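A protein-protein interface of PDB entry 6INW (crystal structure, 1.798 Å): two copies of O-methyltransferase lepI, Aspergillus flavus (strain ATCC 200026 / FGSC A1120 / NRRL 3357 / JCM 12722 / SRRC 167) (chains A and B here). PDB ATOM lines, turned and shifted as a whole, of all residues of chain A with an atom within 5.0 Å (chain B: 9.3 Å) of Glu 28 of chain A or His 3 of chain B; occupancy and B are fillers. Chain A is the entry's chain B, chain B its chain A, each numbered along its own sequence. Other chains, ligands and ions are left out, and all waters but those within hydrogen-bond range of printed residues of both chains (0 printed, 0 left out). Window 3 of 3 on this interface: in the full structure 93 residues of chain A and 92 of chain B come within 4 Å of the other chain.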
ATOM      1  N   PHE A  24      25.711 -19.073 -22.718  1.00  0.00           N
ATOM      2  CA  PHE A  24      25.816 -18.582 -24.090  1.00  0.00           C
ATOM      3  C   PHE A  24      24.979 -19.429 -25.039  1.00  0.00           C
ATOM      4  O   PHE A  24      24.312 -18.897 -25.938  1.00  0.00           O
ATOM      5  CB  PHE A  24      27.282 -18.557 -24.519  1.00  0.00           C
ATOM      6  CG  PHE A  24      28.188 -17.898 -23.515  1.00  0.00           C
ATOM      7  CD1 PHE A  24      27.874 -16.647 -22.997  1.00  0.00           C
ATOM      8  CD2 PHE A  24      29.340 -18.532 -23.073  1.00  0.00           C
ATOM      9  CE1 PHE A  24      28.701 -16.033 -22.067  1.00  0.00           C
ATOM     10  CE2 PHE A  24      30.171 -17.924 -22.141  1.00  0.00           C
ATOM     11  CZ  PHE A  24      29.851 -16.676 -21.637  1.00  0.00           C
ATOM     12  N   GLY A  25      24.993 -20.750 -24.844  1.00  0.00           N
ATOM     13  CA  GLY A  25      24.112 -21.611 -25.615  1.00  0.00           C
ATOM     14  C   GLY A  25      22.645 -21.310 -25.374  1.00  0.00           C
ATOM     15  O   GLY A  25      21.834 -21.345 -26.301  1.00  0.00           O
ATOM     16  N   ARG A  26      22.281 -21.008 -24.123  1.00  0.00           N
ATOM     17  CA  ARG A  26      20.893 -20.659 -23.836  1.00  0.00           C
ATOM     18  C   ARG A  26      20.515 -19.336 -24.491  1.00  0.00           C
ATOM     19  O   ARG A  26      19.387 -19.176 -24.970  1.00  0.00           O
ATOM     20  CB  ARG A  26      20.655 -20.607 -22.327  1.00  0.00           C
ATOM     21  CG  ARG A  26      20.359 -21.968 -21.704  1.00  0.00           C
ATOM     22  CD  ARG A  26      19.930 -21.840 -20.247  1.00  0.00           C
ATOM     23  NE  ARG A  26      21.044 -21.451 -19.389  1.00  0.00           N
ATOM     24  CZ  ARG A  26      22.037 -22.262 -19.042  1.00  0.00           C
ATOM     25  NH1 ARG A  26      22.056 -23.514 -19.478  1.00  0.00           N
ATOM     26  NH2 ARG A  26      23.013 -21.823 -18.260  1.00  0.00           N
ATOM     27  N   ALA A  27      21.442 -18.374 -24.523  1.00  0.00           N
ATOM     28  CA  ALA A  27      21.172 -17.121 -25.224  1.00  0.00           C
ATOM     29  C   ALA A  27      20.963 -17.359 -26.717  1.00  0.00           C
ATOM     30  O   ALA A  27      20.074 -16.756 -27.335  1.00  0.00           O
ATOM     31  CB  ALA A  27      22.312 -16.130 -24.984  1.00  0.00           C
ATOM     32  N   GLU A  28      21.776 -18.235 -27.314  1.00  0.00           N
ATOM     33  CA  GLU A  28      21.594 -18.560 -28.728  1.00  0.00           C
ATOM     34  C   GLU A  28      20.251 -19.244 -28.970  1.00  0.00           C
ATOM     35  O   GLU A  28      19.568 -18.962 -29.965  1.00  0.00           O
ATOM     36  CB  GLU A  28      22.745 -19.440 -29.218  1.00  0.00           C
ATOM     37  CG  GLU A  28      24.073 -18.701 -29.313  1.00  0.00           C
ATOM     38  CD  GLU A  28      24.991 -19.280 -30.368  1.00  0.00           C
ATOM     39  OE1 GLU A  28      24.512 -19.573 -31.483  1.00  0.00           O
ATOM     40  OE2 GLU A  28      26.197 -19.437 -30.081  1.00  0.00           O
ATOM     41  N   ILE A  29      19.854 -20.148 -28.068  1.00  0.00           N
ATOM     42  CA  ILE A  29      18.548 -20.792 -28.198  1.00  0.00           C
ATOM     43  C   ILE A  29      17.430 -19.760 -28.108  1.00  0.00           C
ATOM     44  O   ILE A  29      16.461 -19.808 -28.875  1.00  0.00           O
ATOM     45  CB  ILE A  29      18.377 -21.901 -27.145  1.00  0.00           C
ATOM     46  CG1 ILE A  29      19.265 -23.101 -27.478  1.00  0.00           C
ATOM     47  CG2 ILE A  29      16.912 -22.336 -27.064  1.00  0.00           C
ATOM     48  CD1 ILE A  29      19.332 -24.141 -26.372  1.00  0.00           C
ATOM     49  N   ASN A  30      17.539 -18.814 -27.170  1.00  0.00           N
ATOM     50  CA  ASN A  30      16.494 -17.802 -27.022  1.00  0.00           C
ATOM     51  C   ASN A  30      16.387 -16.920 -28.261  1.00  0.00           C
ATOM     52  O   ASN A  30      15.278 -16.595 -28.713  1.00  0.00           O
ATOM     53  CB  ASN A  30      16.756 -16.950 -25.781  1.00  0.00           C
ATOM     54  CG  ASN A  30      15.868 -17.340 -24.622  1.00  0.00           C
ATOM     55  OD1 ASN A  30      15.396 -18.474 -24.544  1.00  0.00           O
ATOM     56  ND2 ASN A  30      15.625 -16.400 -23.716  1.00  0.00           N
ATOM     57  N   ASP A  31      17.530 -16.511 -28.818  1.00  0.00           N
ATOM     58  CA  ASP A  31      17.502 -15.736 -30.056  1.00  0.00           C
ATOM     59  C   ASP A  31      16.863 -16.537 -31.190  1.00  0.00           C
ATOM     60  O   ASP A  31      16.120 -15.982 -32.014  1.00  0.00           O
ATOM     61  CB  ASP A  31      18.917 -15.297 -30.431  1.00  0.00           C
ATOM     62  CG  ASP A  31      19.402 -14.113 -29.601  1.00  0.00           C
ATOM     63  OD1 ASP A  31      18.589 -13.528 -28.851  1.00  0.00           O
ATOM     64  OD2 ASP A  31      20.598 -13.767 -29.696  1.00  0.00           O
ATOM     65  N   ALA A  32      17.138 -17.844 -31.245  1.00  0.00           N
ATOM     66  CA  ALA A  32      16.514 -18.682 -32.264  1.00  0.00           C
ATOM     67  C   ALA A  32      15.004 -18.772 -32.062  1.00  0.00           C
ATOM     68  O   ALA A  32      14.239 -18.761 -33.033  1.00  0.00           O
ATOM     69  CB  ALA A  32      17.143 -20.077 -32.255  1.00  0.00           C
ATOM     70  N   ARG A 335      22.814  -8.709 -33.280  1.00  0.00           N
ATOM     71  CA  ARG A 335      21.617  -9.164 -32.587  1.00  0.00           C
ATOM     72  C   ARG A 335      20.789  -7.991 -32.071  1.00  0.00           C
ATOM     73  O   ARG A 335      21.260  -6.855 -31.982  1.00  0.00           O
ATOM     74  CB  ARG A 335      21.995 -10.084 -31.429  1.00  0.00           C
ATOM     75  CG  ARG A 335      23.010 -11.155 -31.801  1.00  0.00           C
ATOM     76  CD  ARG A 335      22.357 -12.507 -31.889  1.00  0.00           C
ATOM     77  NE  ARG A 335      23.214 -13.496 -32.532  1.00  0.00           N
ATOM     78  CZ  ARG A 335      22.997 -14.806 -32.470  1.00  0.00           C
ATOM     79  NH1 ARG A 335      21.957 -15.267 -31.790  1.00  0.00           N
ATOM     80  NH2 ARG A 335      23.814 -15.653 -33.082  1.00  0.00           N
ATOM     81  N   PRO A 379      26.084 -14.571 -27.589  1.00  0.00           N
ATOM     82  CA  PRO A 379      26.503 -14.126 -28.924  1.00  0.00           C
ATOM     83  C   PRO A 379      26.608 -12.609 -29.050  1.00  0.00           C
ATOM     84  O   PRO A 379      27.314 -12.133 -29.933  1.00  0.00           O
ATOM     85  CB  PRO A 379      25.397 -14.668 -29.832  1.00  0.00           C
ATOM     86  CG  PRO A 379      24.192 -14.690 -28.959  1.00  0.00           C
ATOM     87  CD  PRO A 379      24.682 -15.025 -27.576  1.00  0.00           C
ATOM     88  N   HIS B   3      26.618 -26.161 -31.447  1.00  0.00           N
ATOM     89  CA  HIS B   3      26.168 -24.839 -31.030  1.00  0.00           C
ATOM     90  C   HIS B   3      25.289 -24.249 -32.125  1.00  0.00           C
ATOM     91  O   HIS B   3      24.095 -24.112 -31.973  1.00  0.00           O
ATOM     92  CB  HIS B   3      27.408 -24.004 -30.631  1.00  0.00           C
ATOM     93  CG  HIS B   3      27.957 -23.135 -31.714  1.00  0.00           C
ATOM     94  ND1 HIS B   3      28.434 -23.630 -32.906  1.00  0.00           N
ATOM     95  CD2 HIS B   3      28.063 -21.795 -31.796  1.00  0.00           C
ATOM     96  CE1 HIS B   3      28.795 -22.635 -33.678  1.00  0.00           C
ATOM     97  NE2 HIS B   3      28.583 -21.507 -33.026  1.00  0.00           N
ATOM     98  N   MET B   4      25.888 -23.987 -33.269  1.00  0.00           N
ATOM     99  CA  MET B   4      25.219 -23.494 -34.454  1.00  0.00           C
ATOM    100  C   MET B   4      24.331 -24.571 -34.995  1.00  0.00           C
ATOM    101  O   MET B   4      23.272 -24.286 -35.506  1.00  0.00           O
ATOM    102  CB  MET B   4      26.225 -23.301 -35.612  1.00  0.00           C
ATOM    103  CG  MET B   4      26.980 -21.998 -35.785  1.00  0.00           C
ATOM    104  SD  MET B   4      27.165 -21.306 -37.654  1.00  0.00           S
ATOM    105  CE  MET B   4      27.163 -23.041 -38.597  1.00  0.00           C
ATOM    106  N   GLU B   5      24.812 -25.788 -34.958  1.00  0.00           N
ATOM    107  CA  GLU B   5      24.114 -26.924 -35.551  1.00  0.00           C
ATOM    108  C   GLU B   5      22.840 -27.288 -34.805  1.00  0.00           C
ATOM    109  O   GLU B   5      21.879 -27.627 -35.367  1.00  0.00           O
ATOM    110  CB  GLU B   5      25.034 -28.131 -35.671  1.00  0.00           C
ATOM    111  CG  GLU B   5      24.519 -29.266 -36.525  1.00  0.00           C
ATOM    112  CD  GLU B   5      25.230 -30.575 -36.224  1.00  0.00           C
ATOM    113  OE1 GLU B   5      26.417 -30.490 -35.958  1.00  0.00           O
ATOM    114  OE2 GLU B   5      24.646 -31.678 -36.236  1.00  0.00           O
ATOM    115  N   THR B   6      22.922 -27.219 -33.501  1.00  0.00           N
ATOM    116  CA  THR B   6      21.780 -27.451 -32.673  1.00  0.00           C
ATOM    117  C   THR B   6      20.684 -26.403 -32.912  1.00  0.00           C
ATOM    118  O   THR B   6      19.559 -26.710 -33.055  1.00  0.00           O
ATOM    119  CB  THR B   6      22.212 -27.411 -31.221  1.00  0.00           C
ATOM    120  OG1 THR B   6      23.056 -28.483 -30.996  1.00  0.00           O
ATOM    121  CG2 THR B   6      21.086 -27.504 -30.308  1.00  0.00           C
ATOM    122  N   VAL B   7      21.087 -25.160 -33.006  1.00  0.00           N
ATOM    123  CA  VAL B   7      20.171 -24.085 -33.270  1.00  0.00           C
ATOM    124  C   VAL B   7      19.520 -24.270 -34.633  1.00  0.00           C
ATOM    125  O   VAL B   7      18.366 -24.124 -34.784  1.00  0.00           O
ATOM    126  CB  VAL B   7      20.917 -22.738 -33.197  1.00  0.00           C
ATOM    127  CG1 VAL B   7      20.215 -21.622 -33.885  1.00  0.00           C
ATOM    128  CG2 VAL B   7      21.201 -22.379 -31.797  1.00  0.00           C
ATOM    129  N   ALA B   8      20.315 -24.559 -35.635  1.00  0.00           N
ATOM    130  CA  ALA B   8      19.735 -24.779 -36.956  1.00  0.00           C
ATOM    131  C   ALA B   8      18.761 -25.951 -36.944  1.00  0.00           C
ATOM    132  O   ALA B   8      17.737 -25.924 -37.637  1.00  0.00           O
ATOM    133  CB  ALA B   8      20.842 -25.011 -37.985  1.00  0.00           C
ATOM    134  N   ALA B   9      19.065 -26.992 -36.164  1.00  0.00           N
ATOM    135  CA  ALA B   9      18.182 -28.151 -36.102  1.00  0.00           C
ATOM    136  C   ALA B   9      16.869 -27.813 -35.409  1.00  0.00           C
ATOM    137  O   ALA B   9      15.805 -28.284 -35.826  1.00  0.00           O
ATOM    138  CB  ALA B   9      18.880 -29.312 -35.395  1.00  0.00           C
ATOM    139  N   ILE B  10      16.923 -27.014 -34.341  1.00  0.00           N
ATOM    140  CA  ILE B  10      15.694 -26.555 -33.694  1.00  0.00           C
ATOM    141  C   ILE B  10      14.827 -25.801 -34.691  1.00  0.00           C
ATOM    142  O   ILE B  10      13.617 -26.032 -34.791  1.00  0.00           O
ATOM    143  CB  ILE B  10      16.017 -25.681 -32.470  1.00  0.00           C
ATOM    144  CG1 ILE B  10      16.705 -26.501 -31.378  1.00  0.00           C
ATOM    145  CG2 ILE B  10      14.747 -25.038 -31.935  1.00  0.00           C
ATOM    146  CD1 ILE B  10      17.176 -25.662 -30.207  1.00  0.00           C
ATOM    147  N   LYS B  11      15.437 -24.886 -35.450  1.00  0.00           N
ATOM    148  CA  LYS B  11      14.689 -24.122 -36.443  1.00  0.00           C
ATOM    149  C   LYS B  11      14.071 -25.037 -37.488  1.00  0.00           C
ATOM    150  O   LYS B  11      12.889 -24.902 -37.825  1.00  0.00           O
ATOM    151  CB  LYS B  11      15.602 -23.087 -37.102  1.00  0.00           C
ATOM    152  CG  LYS B  11      16.045 -21.982 -36.167  1.00  0.00           C
ATOM    153  CD  LYS B  11      16.784 -20.885 -36.915  1.00  0.00           C
ATOM    154  CE  LYS B  11      17.562 -20.005 -35.953  1.00  0.00           C
ATOM    155  NZ  LYS B  11      18.354 -18.959 -36.659  1.00  0.00           N
ATOM    156  N   LEU B  40      13.237 -19.041 -20.234  1.00  0.00           N
ATOM    157  CA  LEU B  40      14.660 -19.339 -20.347  1.00  0.00           C
ATOM    158  C   LEU B  40      15.561 -18.108 -20.294  1.00  0.00           C
ATOM    159  O   LEU B  40      16.780 -18.262 -20.176  1.00  0.00           O
ATOM    160  CB  LEU B  40      14.929 -20.115 -21.640  1.00  0.00           C
ATOM    161  CG  LEU B  40      14.344 -21.530 -21.645  1.00  0.00           C
ATOM    162  CD1 LEU B  40      14.551 -22.203 -22.992  1.00  0.00           C
ATOM    163  CD2 LEU B  40      14.950 -22.366 -20.522  1.00  0.00           C
ATOM    164  N   ASP B  45      18.379 -10.399 -19.147  1.00  0.00           N
ATOM    165  CA  ASP B  45      17.692 -10.528 -20.429  1.00  0.00           C
ATOM    166  C   ASP B  45      16.259 -10.023 -20.344  1.00  0.00           C
ATOM    167  O   ASP B  45      15.761  -9.400 -21.284  1.00  0.00           O
ATOM    168  CB  ASP B  45      17.699 -11.985 -20.898  1.00  0.00           C
ATOM    169  CG  ASP B  45      19.046 -12.431 -21.427  1.00  0.00           C
ATOM    170  OD1 ASP B  45      19.941 -11.576 -21.599  1.00  0.00           O
ATOM    171  OD2 ASP B  45      19.207 -13.650 -21.662  1.00  0.00           O
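OE2 of Glu 28 of chain A touches CD2 of His 3 of chain B (3.5 Å).
Leu 40 of chain B touches Asn 30 of chain A.
Val 7 of chain B touches Ala 32 of chain A.
Ala 32 of chain A touches Lys 11 of chain B (CB to CE, 3.7 Å).
No position is printed for both chains.
Of the 4 pairs that touch across the chains among the printed residues, none has its exchanged pair printed and touching as well.
Hydrophobic or aromatic side chains of chain B that line the printed part of chain A: His 3, Val 7 and Leu 40.
Of the 11 printed residues of chain A, 3 touch a printed residue of chain B.
Among the printed residues, 4 pairs touch across the chains.
Among the printed residues, no Asp or Glu carboxylate lies within 4 Å of a Lys or Arg side-chain nitrogen of the other chain.
Glu 28 of chain A touches just one residue of chain B: His 3.
Of chain A, only Glu 28 comes within 4 Å of His 3 of chain B.
No residue of chain B comes within 4 Å of Ala 27 of chain A.
Of the printed residues of chain B, Asn 30 of chain A touches Leu 40.
Of the printed residues of chain B, Ala 32 of chain A touches Val 7 (3.8 Å) and Lys 11 (3.7 Å).
Of the printed residues of chain A, Leu 40 of chain B touches Asn 30 (3.4 Å).
Of the printed residues of chain A, Lys 11 of chain B touches Ala 32.
Printed residues of chain A within 4 Å of Val 7 of chain B: Ala 32 (3.8 Å).
Arg 335 of chain A touches none of the printed residues of chain B.
The nearest residue of chain B that does not touch Glu 28 of chain A is Val 7 of chain B (4.2 Å).
The nearest printed residue of chain B that does not touch Ala 32 of chain A is Ile 10 of chain B (5.5 Å).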
